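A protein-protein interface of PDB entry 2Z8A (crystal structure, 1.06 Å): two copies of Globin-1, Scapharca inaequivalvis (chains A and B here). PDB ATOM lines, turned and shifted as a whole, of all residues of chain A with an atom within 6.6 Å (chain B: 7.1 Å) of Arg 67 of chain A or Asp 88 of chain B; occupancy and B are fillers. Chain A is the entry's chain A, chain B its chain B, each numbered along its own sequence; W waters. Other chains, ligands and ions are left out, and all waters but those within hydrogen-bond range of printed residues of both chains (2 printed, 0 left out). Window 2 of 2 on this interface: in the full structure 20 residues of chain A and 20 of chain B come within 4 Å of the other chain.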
ATOM      1  N   LYS A  30     -29.346 -33.135  27.162  1.00  0.00           N
ATOM      2  CA  LYS A  30     -28.565 -32.147  27.906  1.00  0.00           C
ATOM      3  C   LYS A  30     -29.127 -31.923  29.304  1.00  0.00           C
ATOM      4  O   LYS A  30     -28.429 -32.025  30.318  1.00  0.00           O
ATOM      5  CB  LYS A  30     -28.529 -30.834  27.124  1.00  0.00           C
ATOM      6  CG  LYS A  30     -27.925 -29.660  27.872  1.00  0.00           C
ATOM      7  CD  LYS A  30     -27.697 -28.482  26.942  1.00  0.00           C
ATOM      8  CE  LYS A  30     -28.986 -27.775  26.570  1.00  0.00           C
ATOM      9  NZ  LYS A  30     -28.752 -26.679  25.586  1.00  0.00           N
ATOM     10  N   VAL A  34     -27.332 -33.719  32.617  1.00  0.00           N
ATOM     11  CA  VAL A  34     -26.731 -32.903  33.673  1.00  0.00           C
ATOM     12  C   VAL A  34     -27.450 -33.144  34.996  1.00  0.00           C
ATOM     13  O   VAL A  34     -26.806 -33.232  36.044  1.00  0.00           O
ATOM     14  CB  VAL A  34     -26.732 -31.410  33.300  1.00  0.00           C
ATOM     15  CG1 VAL A  34     -26.333 -30.543  34.481  1.00  0.00           C
ATOM     16  CG2 VAL A  34     -25.795 -31.171  32.122  1.00  0.00           C
ATOM     17  N   GLY A  60     -22.616 -27.318  37.682  1.00  0.00           N
ATOM     18  CA  GLY A  60     -23.685 -27.913  36.900  1.00  0.00           C
ATOM     19  C   GLY A  60     -23.680 -27.495  35.443  1.00  0.00           C
ATOM     20  O   GLY A  60     -22.662 -27.601  34.759  1.00  0.00           O
ATOM     21  N   MET A  61     -24.821 -27.020  34.956  1.00  0.00           N
ATOM     22  CA  MET A  61     -25.021 -26.732  33.540  1.00  0.00           C
ATOM     23  C   MET A  61     -24.054 -25.670  33.035  1.00  0.00           C
ATOM     24  O   MET A  61     -23.740 -25.622  31.842  1.00  0.00           O
ATOM     25  CB  MET A  61     -26.466 -26.288  33.306  1.00  0.00           C
ATOM     26  CG  MET A  61     -26.855 -26.078  31.856  1.00  0.00           C
ATOM     27  SD  MET A  61     -26.889 -27.606  30.905  1.00  0.00           S
ATOM     28  CE  MET A  61     -28.286 -28.447  31.641  1.00  0.00           C
ATOM     29  N   ALA A  62     -23.577 -24.818  33.935  1.00  0.00           N
ATOM     30  CA  ALA A  62     -22.705 -23.711  33.562  1.00  0.00           C
ATOM     31  C   ALA A  62     -21.285 -24.183  33.266  1.00  0.00           C
ATOM     32  O   ALA A  62     -20.483 -23.447  32.689  1.00  0.00           O
ATOM     33  CB  ALA A  62     -22.698 -22.659  34.662  1.00  0.00           C
ATOM     34  N   ASN A  63     -20.984 -25.411  33.666  1.00  0.00           N
ATOM     35  CA  ASN A  63     -19.685 -26.034  33.445  1.00  0.00           C
ATOM     36  C   ASN A  63     -19.657 -26.733  32.093  1.00  0.00           C
ATOM     37  O   ASN A  63     -20.291 -27.774  31.922  1.00  0.00           O
ATOM     38  CB  ASN A  63     -19.395 -27.012  34.577  1.00  0.00           C
ATOM     39  CG  ASN A  63     -18.068 -27.722  34.495  1.00  0.00           C
ATOM     40  OD1 ASN A  63     -17.547 -28.002  33.416  1.00  0.00           O
ATOM     41  ND2 ASN A  63     -17.498 -28.030  35.657  1.00  0.00           N
ATOM     42  N   ASP A  64     -18.932 -26.173  31.132  1.00  0.00           N
ATOM     43  CA  ASP A  64     -18.932 -26.666  29.761  1.00  0.00           C
ATOM     44  C   ASP A  64     -18.451 -28.111  29.677  1.00  0.00           C
ATOM     45  O   ASP A  64     -19.024 -28.918  28.941  1.00  0.00           O
ATOM     46  CB  ASP A  64     -18.049 -25.800  28.866  1.00  0.00           C
ATOM     47  CG  ASP A  64     -18.620 -24.437  28.548  1.00  0.00           C
ATOM     48  OD1 ASP A  64     -19.843 -24.229  28.680  1.00  0.00           O
ATOM     49  OD2 ASP A  64     -17.821 -23.556  28.158  1.00  0.00           O
ATOM     50  N   LYS A  65     -17.398 -28.449  30.415  1.00  0.00           N
ATOM     51  CA  LYS A  65     -16.893 -29.820  30.378  1.00  0.00           C
ATOM     52  C   LYS A  65     -17.912 -30.788  30.964  1.00  0.00           C
ATOM     53  O   LYS A  65     -18.100 -31.889  30.445  1.00  0.00           O
ATOM     54  CB  LYS A  65     -15.562 -29.926  31.123  1.00  0.00           C
ATOM     55  CG  LYS A  65     -14.389 -29.341  30.347  1.00  0.00           C
ATOM     56  CD  LYS A  65     -13.072 -29.522  31.075  1.00  0.00           C
ATOM     57  CE  LYS A  65     -11.903 -29.000  30.256  1.00  0.00           C
ATOM     58  NZ  LYS A  65     -11.727 -27.530  30.413  1.00  0.00           N
ATOM     59  N   LEU A  66     -18.583 -30.394  32.043  1.00  0.00           N
ATOM     60  CA  LEU A  66     -19.637 -31.246  32.592  1.00  0.00           C
ATOM     61  C   LEU A  66     -20.790 -31.397  31.607  1.00  0.00           C
ATOM     62  O   LEU A  66     -21.357 -32.483  31.485  1.00  0.00           O
ATOM     63  CB  LEU A  66     -20.152 -30.697  33.922  1.00  0.00           C
ATOM     64  CG  LEU A  66     -21.263 -31.505  34.602  1.00  0.00           C
ATOM     65  CD1 LEU A  66     -20.849 -32.951  34.830  1.00  0.00           C
ATOM     66  CD2 LEU A  66     -21.651 -30.839  35.912  1.00  0.00           C
ATOM     67  N   ARG A  67     -21.146 -30.319  30.912  1.00  0.00           N
ATOM     68  CA  ARG A  67     -22.228 -30.415  29.934  1.00  0.00           C
ATOM     69  C   ARG A  67     -21.867 -31.381  28.812  1.00  0.00           C
ATOM     70  O   ARG A  67     -22.679 -32.215  28.420  1.00  0.00           O
ATOM     71  CB  ARG A  67     -22.565 -29.039  29.357  1.00  0.00           C
ATOM     72  CG  ARG A  67     -23.995 -28.940  28.846  1.00  0.00           C
ATOM     73  CD  ARG A  67     -24.351 -27.482  28.586  1.00  0.00           C
ATOM     74  NE  ARG A  67     -23.478 -26.896  27.580  1.00  0.00           N
ATOM     75  CZ  ARG A  67     -22.511 -26.010  27.739  1.00  0.00           C
ATOM     76  NH1 ARG A  67     -22.181 -25.497  28.917  1.00  0.00           N
ATOM     77  NH2 ARG A  67     -21.829 -25.606  26.669  1.00  0.00           N
ATOM     78  N   GLY A  68     -20.645 -31.277  28.292  1.00  0.00           N
ATOM     79  CA  GLY A  68     -20.224 -32.168  27.220  1.00  0.00           C
ATOM     80  C   GLY A  68     -20.176 -33.620  27.653  1.00  0.00           C
ATOM     81  O   GLY A  68     -20.594 -34.520  26.924  1.00  0.00           O
ATOM     82  N   HIS A  69     -19.662 -33.857  28.855  1.00  0.00           N
ATOM     83  CA  HIS A  69     -19.660 -35.182  29.456  1.00  0.00           C
ATOM     84  C   HIS A  69     -21.076 -35.737  29.574  1.00  0.00           C
ATOM     85  O   HIS A  69     -21.344 -36.896  29.261  1.00  0.00           O
ATOM     86  CB  HIS A  69     -18.981 -35.129  30.835  1.00  0.00           C
ATOM     87  CG  HIS A  69     -19.277 -36.353  31.650  1.00  0.00           C
ATOM     88  ND1 HIS A  69     -18.568 -37.524  31.501  1.00  0.00           N
ATOM     89  CD2 HIS A  69     -20.202 -36.585  32.612  1.00  0.00           C
ATOM     90  CE1 HIS A  69     -19.056 -38.418  32.340  1.00  0.00           C
ATOM     91  NE2 HIS A  69     -20.051 -37.878  33.025  1.00  0.00           N
ATOM     92  N   SER A  70     -21.983 -34.907  30.076  1.00  0.00           N
ATOM     93  CA  SER A  70     -23.319 -35.361  30.442  1.00  0.00           C
ATOM     94  C   SER A  70     -24.153 -35.695  29.211  1.00  0.00           C
ATOM     95  O   SER A  70     -24.877 -36.691  29.167  1.00  0.00           O
ATOM     96  CB  SER A  70     -24.031 -34.297  31.280  1.00  0.00           C
ATOM     97  OG  SER A  70     -23.371 -34.076  32.507  1.00  0.00           O
ATOM     98  N   ILE A  71     -24.062 -34.845  28.187  1.00  0.00           N
ATOM     99  CA  ILE A  71     -24.719 -35.160  26.919  1.00  0.00           C
ATOM    100  C   ILE A  71     -24.204 -36.486  26.377  1.00  0.00           C
ATOM    101  O   ILE A  71     -24.965 -37.355  25.955  1.00  0.00           O
ATOM    102  CB  ILE A  71     -24.515 -34.030  25.893  1.00  0.00           C
ATOM    103  CG1 ILE A  71     -25.191 -32.719  26.301  1.00  0.00           C
ATOM    104  CG2 ILE A  71     -24.964 -34.466  24.510  1.00  0.00           C
ATOM    105  CD1 ILE A  71     -24.714 -31.505  25.542  1.00  0.00           C
ATOM    106  N   THR A  72     -22.881 -36.641  26.397  1.00  0.00           N
ATOM    107  CA  THR A  72     -22.276 -37.848  25.835  1.00  0.00           C
ATOM    108  C   THR A  72     -22.685 -39.089  26.614  1.00  0.00           C
ATOM    109  O   THR A  72     -22.914 -40.152  26.020  1.00  0.00           O
ATOM    110  CB  THR A  72     -20.746 -37.674  25.789  1.00  0.00           C
ATOM    111  OG1 THR A  72     -20.454 -36.569  24.915  1.00  0.00           O
ATOM    112  CG2 THR A  72     -20.070 -38.898  25.208  1.00  0.00           C
ATOM    113  N   TYR B   4     -15.553 -22.585  18.637  1.00  0.00           N
ATOM    114  CA  TYR B   4     -16.864 -21.959  18.523  1.00  0.00           C
ATOM    115  C   TYR B   4     -16.994 -21.297  17.154  1.00  0.00           C
ATOM    116  O   TYR B   4     -18.044 -21.398  16.524  1.00  0.00           O
ATOM    117  CB  TYR B   4     -17.106 -20.946  19.642  1.00  0.00           C
ATOM    118  CG  TYR B   4     -18.478 -20.315  19.574  1.00  0.00           C
ATOM    119  CD1 TYR B   4     -19.593 -20.934  20.126  1.00  0.00           C
ATOM    120  CD2 TYR B   4     -18.662 -19.090  18.944  1.00  0.00           C
ATOM    121  CE1 TYR B   4     -20.843 -20.349  20.056  1.00  0.00           C
ATOM    122  CE2 TYR B   4     -19.907 -18.498  18.869  1.00  0.00           C
ATOM    123  CZ  TYR B   4     -20.996 -19.131  19.427  1.00  0.00           C
ATOM    124  OH  TYR B   4     -22.240 -18.543  19.354  1.00  0.00           O
ATOM    125  N   ALA B   7     -17.708 -23.947  14.681  1.00  0.00           N
ATOM    126  CA  ALA B   7     -19.073 -24.442  14.861  1.00  0.00           C
ATOM    127  C   ALA B   7     -20.106 -23.437  14.366  1.00  0.00           C
ATOM    128  O   ALA B   7     -21.104 -23.800  13.740  1.00  0.00           O
ATOM    129  CB  ALA B   7     -19.320 -24.788  16.323  1.00  0.00           C
ATOM    130  N   GLN B  83     -26.455 -31.804  17.784  1.00  0.00           N
ATOM    131  CA  GLN B  83     -26.107 -30.522  18.385  1.00  0.00           C
ATOM    132  C   GLN B  83     -25.919 -29.406  17.359  1.00  0.00           C
ATOM    133  O   GLN B  83     -25.578 -28.286  17.752  1.00  0.00           O
ATOM    134  CB  GLN B  83     -24.817 -30.607  19.207  1.00  0.00           C
ATOM    135  CG  GLN B  83     -24.714 -31.691  20.245  1.00  0.00           C
ATOM    136  CD  GLN B  83     -26.007 -31.992  20.968  1.00  0.00           C
ATOM    137  OE1 GLN B  83     -26.756 -31.089  21.337  1.00  0.00           O
ATOM    138  NE2 GLN B  83     -26.258 -33.279  21.176  1.00  0.00           N
ATOM    139  N   ASP B  85     -27.574 -27.257  15.737  1.00  0.00           N
ATOM    140  CA  ASP B  85     -28.280 -25.979  15.780  1.00  0.00           C
ATOM    141  C   ASP B  85     -27.859 -25.136  16.977  1.00  0.00           C
ATOM    142  O   ASP B  85     -28.214 -23.959  17.051  1.00  0.00           O
ATOM    143  CB  ASP B  85     -29.795 -26.200  15.813  1.00  0.00           C
ATOM    144  CG  ASP B  85     -30.361 -26.602  14.467  1.00  0.00           C
ATOM    145  OD1 ASP B  85     -29.696 -26.376  13.434  1.00  0.00           O
ATOM    146  OD2 ASP B  85     -31.482 -27.153  14.439  1.00  0.00           O
ATOM    147  N   ASN B  86     -27.112 -25.716  17.908  1.00  0.00           N
ATOM    148  CA  ASN B  86     -26.643 -24.985  19.081  1.00  0.00           C
ATOM    149  C   ASN B  86     -25.128 -25.101  19.197  1.00  0.00           C
ATOM    150  O   ASN B  86     -24.605 -26.044  19.795  1.00  0.00           O
ATOM    151  CB  ASN B  86     -27.325 -25.491  20.351  1.00  0.00           C
ATOM    152  CG  ASN B  86     -27.015 -24.631  21.561  1.00  0.00           C
ATOM    153  OD1 ASN B  86     -25.913 -24.102  21.690  1.00  0.00           O
ATOM    154  ND2 ASN B  86     -27.988 -24.481  22.451  1.00  0.00           N
ATOM    155  N   PRO B  87     -24.415 -24.149  18.610  1.00  0.00           N
ATOM    156  CA  PRO B  87     -22.948 -24.157  18.665  1.00  0.00           C
ATOM    157  C   PRO B  87     -22.380 -24.320  20.069  1.00  0.00           C
ATOM    158  O   PRO B  87     -21.332 -24.961  20.201  1.00  0.00           O
ATOM    159  CB  PRO B  87     -22.581 -22.773  18.114  1.00  0.00           C
ATOM    160  CG  PRO B  87     -23.695 -22.476  17.161  1.00  0.00           C
ATOM    161  CD  PRO B  87     -24.931 -23.011  17.833  1.00  0.00           C
ATOM    162  N   ASP B  88     -23.015 -23.776  21.101  1.00  0.00           N
ATOM    163  CA  ASP B  88     -22.544 -23.975  22.471  1.00  0.00           C
ATOM    164  C   ASP B  88     -22.456 -25.458  22.814  1.00  0.00           C
ATOM    165  O   ASP B  88     -21.489 -25.972  23.377  1.00  0.00           O
ATOM    166  CB  ASP B  88     -23.463 -23.279  23.474  1.00  0.00           C
ATOM    167  CG  ASP B  88     -23.496 -21.773  23.359  1.00  0.00           C
ATOM    168  OD1 ASP B  88     -22.409 -21.165  23.281  1.00  0.00           O
ATOM    169  OD2 ASP B  88     -24.604 -21.191  23.355  1.00  0.00           O
ATOM    170  N   ASP B  89     -23.528 -26.169  22.460  1.00  0.00           N
ATOM    171  CA  ASP B  89     -23.606 -27.594  22.773  1.00  0.00           C
ATOM    172  C   ASP B  89     -22.664 -28.385  21.874  1.00  0.00           C
ATOM    173  O   ASP B  89     -21.999 -29.317  22.325  1.00  0.00           O
ATOM    174  CB  ASP B  89     -25.047 -28.087  22.638  1.00  0.00           C
ATOM    175  CG  ASP B  89     -25.952 -27.532  23.722  1.00  0.00           C
ATOM    176  OD1 ASP B  89     -25.432 -26.988  24.718  1.00  0.00           O
ATOM    177  OD2 ASP B  89     -27.187 -27.640  23.574  1.00  0.00           O
ATOM    178  N   LEU B  90     -22.594 -28.016  20.594  1.00  0.00           N
ATOM    179  CA  LEU B  90     -21.676 -28.713  19.696  1.00  0.00           C
ATOM    180  C   LEU B  90     -20.240 -28.574  20.185  1.00  0.00           C
ATOM    181  O   LEU B  90     -19.485 -29.547  20.217  1.00  0.00           O
ATOM    182  CB  LEU B  90     -21.789 -28.196  18.261  1.00  0.00           C
ATOM    183  CG  LEU B  90     -20.892 -28.902  17.239  1.00  0.00           C
ATOM    184  CD1 LEU B  90     -21.220 -30.384  17.155  1.00  0.00           C
ATOM    185  CD2 LEU B  90     -21.016 -28.246  15.872  1.00  0.00           C
ATOM    186  N   VAL B  91     -19.848 -27.362  20.575  1.00  0.00           N
ATOM    187  CA  VAL B  91     -18.473 -27.146  21.021  1.00  0.00           C
ATOM    188  C   VAL B  91     -18.167 -28.020  22.228  1.00  0.00           C
ATOM    189  O   VAL B  91     -17.098 -28.626  22.302  1.00  0.00           O
ATOM    190  CB  VAL B  91     -18.201 -25.666  21.346  1.00  0.00           C
ATOM    191  CG1 VAL B  91     -16.868 -25.505  22.061  1.00  0.00           C
ATOM    192  CG2 VAL B  91     -18.232 -24.830  20.076  1.00  0.00           C
ATOM    193  N   CYS B  92     -19.085 -28.110  23.194  1.00  0.00           N
ATOM    194  CA  CYS B  92     -18.682 -28.824  24.416  1.00  0.00           C
ATOM    195  C   CYS B  92     -18.584 -30.323  24.148  1.00  0.00           C
ATOM    196  O   CYS B  92     -17.749 -30.987  24.776  1.00  0.00           O
ATOM    197  CB  CYS B  92     -19.609 -28.504  25.581  1.00  0.00           C
ATOM    198  SG  CYS B  92     -21.257 -29.213  25.587  1.00  0.00           S
ATOM    199  N   VAL B  93     -19.380 -30.888  23.241  1.00  0.00           N
ATOM    200  CA  VAL B  93     -19.195 -32.320  22.967  1.00  0.00           C
ATOM    201  C   VAL B  93     -17.998 -32.540  22.045  1.00  0.00           C
ATOM    202  O   VAL B  93     -17.273 -33.534  22.202  1.00  0.00           O
ATOM    203  CB  VAL B  93     -20.460 -32.988  22.398  1.00  0.00           C
ATOM    204  CG1 VAL B  93     -21.590 -32.902  23.421  1.00  0.00           C
ATOM    205  CG2 VAL B  93     -20.904 -32.391  21.076  1.00  0.00           C
ATOM    206  N   GLU B  95     -15.262 -30.798  22.162  1.00  0.00           N
ATOM    207  CA  GLU B  95     -14.100 -30.686  23.044  1.00  0.00           C
ATOM    208  C   GLU B  95     -13.913 -31.953  23.871  1.00  0.00           C
ATOM    209  O   GLU B  95     -12.773 -32.346  24.136  1.00  0.00           O
ATOM    210  CB  GLU B  95     -14.232 -29.454  23.945  1.00  0.00           C
ATOM    211  CG  GLU B  95     -13.937 -28.148  23.219  1.00  0.00           C
ATOM    212  CD  GLU B  95     -13.987 -26.945  24.137  1.00  0.00           C
ATOM    213  OE1 GLU B  95     -14.978 -26.800  24.883  1.00  0.00           O
ATOM    214  OE2 GLU B  95     -13.031 -26.140  24.111  1.00  0.00           O
HETATM  215  O   HOH W   1     -13.017 -27.283  27.239  1.00  0.00           O
HETATM  216  O   HOH W   2     -19.549 -24.837  25.075  1.00  0.00           O
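Of the 15 printed residues of chain A, 5 touch a printed residue of chain B. Hydrophobic or aromatic side chains of chain B that line the printed part of chain A: Val 93.
The backbone carbonyl oxygen (O) of Met 61 of chain A sits at hydrogen-bond distance from the guanidinium group (NH1) of Arg 67 of chain A (3.3 Å). OD1 of Asp 64 of chain A is in salt-bridge range of NH1 of Arg 67 of chain A (2.7 Å). O of Gly 68 of chain A is in hydrogen-bond range of OG1 of Thr 72 of chain A. OD1 of Asn 86 of chain B lies within hydrogen-bond range of N of Asp 88 of chain B (3.0 Å). The side-chain amide oxygen (OD1) of Asn 86 of chain B sits at hydrogen-bond distance from the backbone NH (N) of Asp 89 of chain B (3.2 Å). The side-chain sulfur of Cys 92 of chain B is in hydrogen-bond range of the backbone carbonyl oxygen of Asp 89 of chain B, 3.3 Å away.
Among the printed residues, pairs that only touch across the chains: Lys 30 of chain A with Asn 86 of chain B (3.9 Å), Asp 64 of chain A with Cys 92 of chain B (3.4 Å), Gly 68 of chain A with Val 93 of chain B (3.99 Å), Ile 71 of chain A with Gln 83 of chain B (3.8 Å) and Ile 71 of chain A with Val 93 of chain B (3.9 Å).
NZ of Lys 30 of chain A lies within salt-bridge range of OD2 of Asp 89 of chain B. The backbone carbonyl oxygen (O) of Asp 88 of chain B sits at hydrogen-bond distance from the guanidinium group (NH2) of Arg 67 of chain A, 3.3 Å away. The guanidinium group (NE) of Arg 67 of chain A lies within salt-bridge range of the side-chain carboxylate (OD1) of Asp 89 of chain B, at 3.5 Å. The side-chain sulfur of Cys 92 of chain B lies within hydrogen-bond range of the guanidinium group of Arg 67 of chain A. The side-chain sulfur of Cys 92 of chain B sits at hydrogen-bond distance from the backbone NH of Gly 68 of chain A (3.5 Å).
Asp 88 of chain B touches just one residue of chain A: Arg 67 (3.3 Å). Printed residues of chain B within 4 Å of Lys 30 of chain A: Asn 86 (3.9 Å) and Asp 89 (2.7 Å). Printed residues of chain A within 4 Å of Gln 83 of chain B: Ile 71. Of the printed residues of chain B, Ile 71 of chain A touches Gln 83 and Val 93. Printed residues of chain A within 4 Å of Asp 89 of chain B: Lys 30 and Arg 67. Of the printed residues of chain B, Gly 68 of chain A touches Cys 92 and Val 93. Val 91 of chain B touches none of the printed residues of chain A. Ala 62 of chain A touches none of the printed residues of chain B. The nearest printed residue of chain A that does not touch Gln 83 of chain B is Lys 30 of chain A (6.1 Å).
Water W2 lies within hydrogen-bond range of the backbone carbonyl oxygen of Asp 88 of chain B (2.8 Å) and the guanidinium group of Arg 67 of chain A (2.9 Å). Water W1 lies within hydrogen-bond range of the side-chain carboxylate (OE1) of Glu 95 of chain B (3.1 Å) and the side-chain amino group (NZ) of Lys 65 of chain A (3.4 Å).
No position is printed for both chains. Of the 10 pairs that touch across the chains among the printed residues, none has its exchanged pair printed and touching as well.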
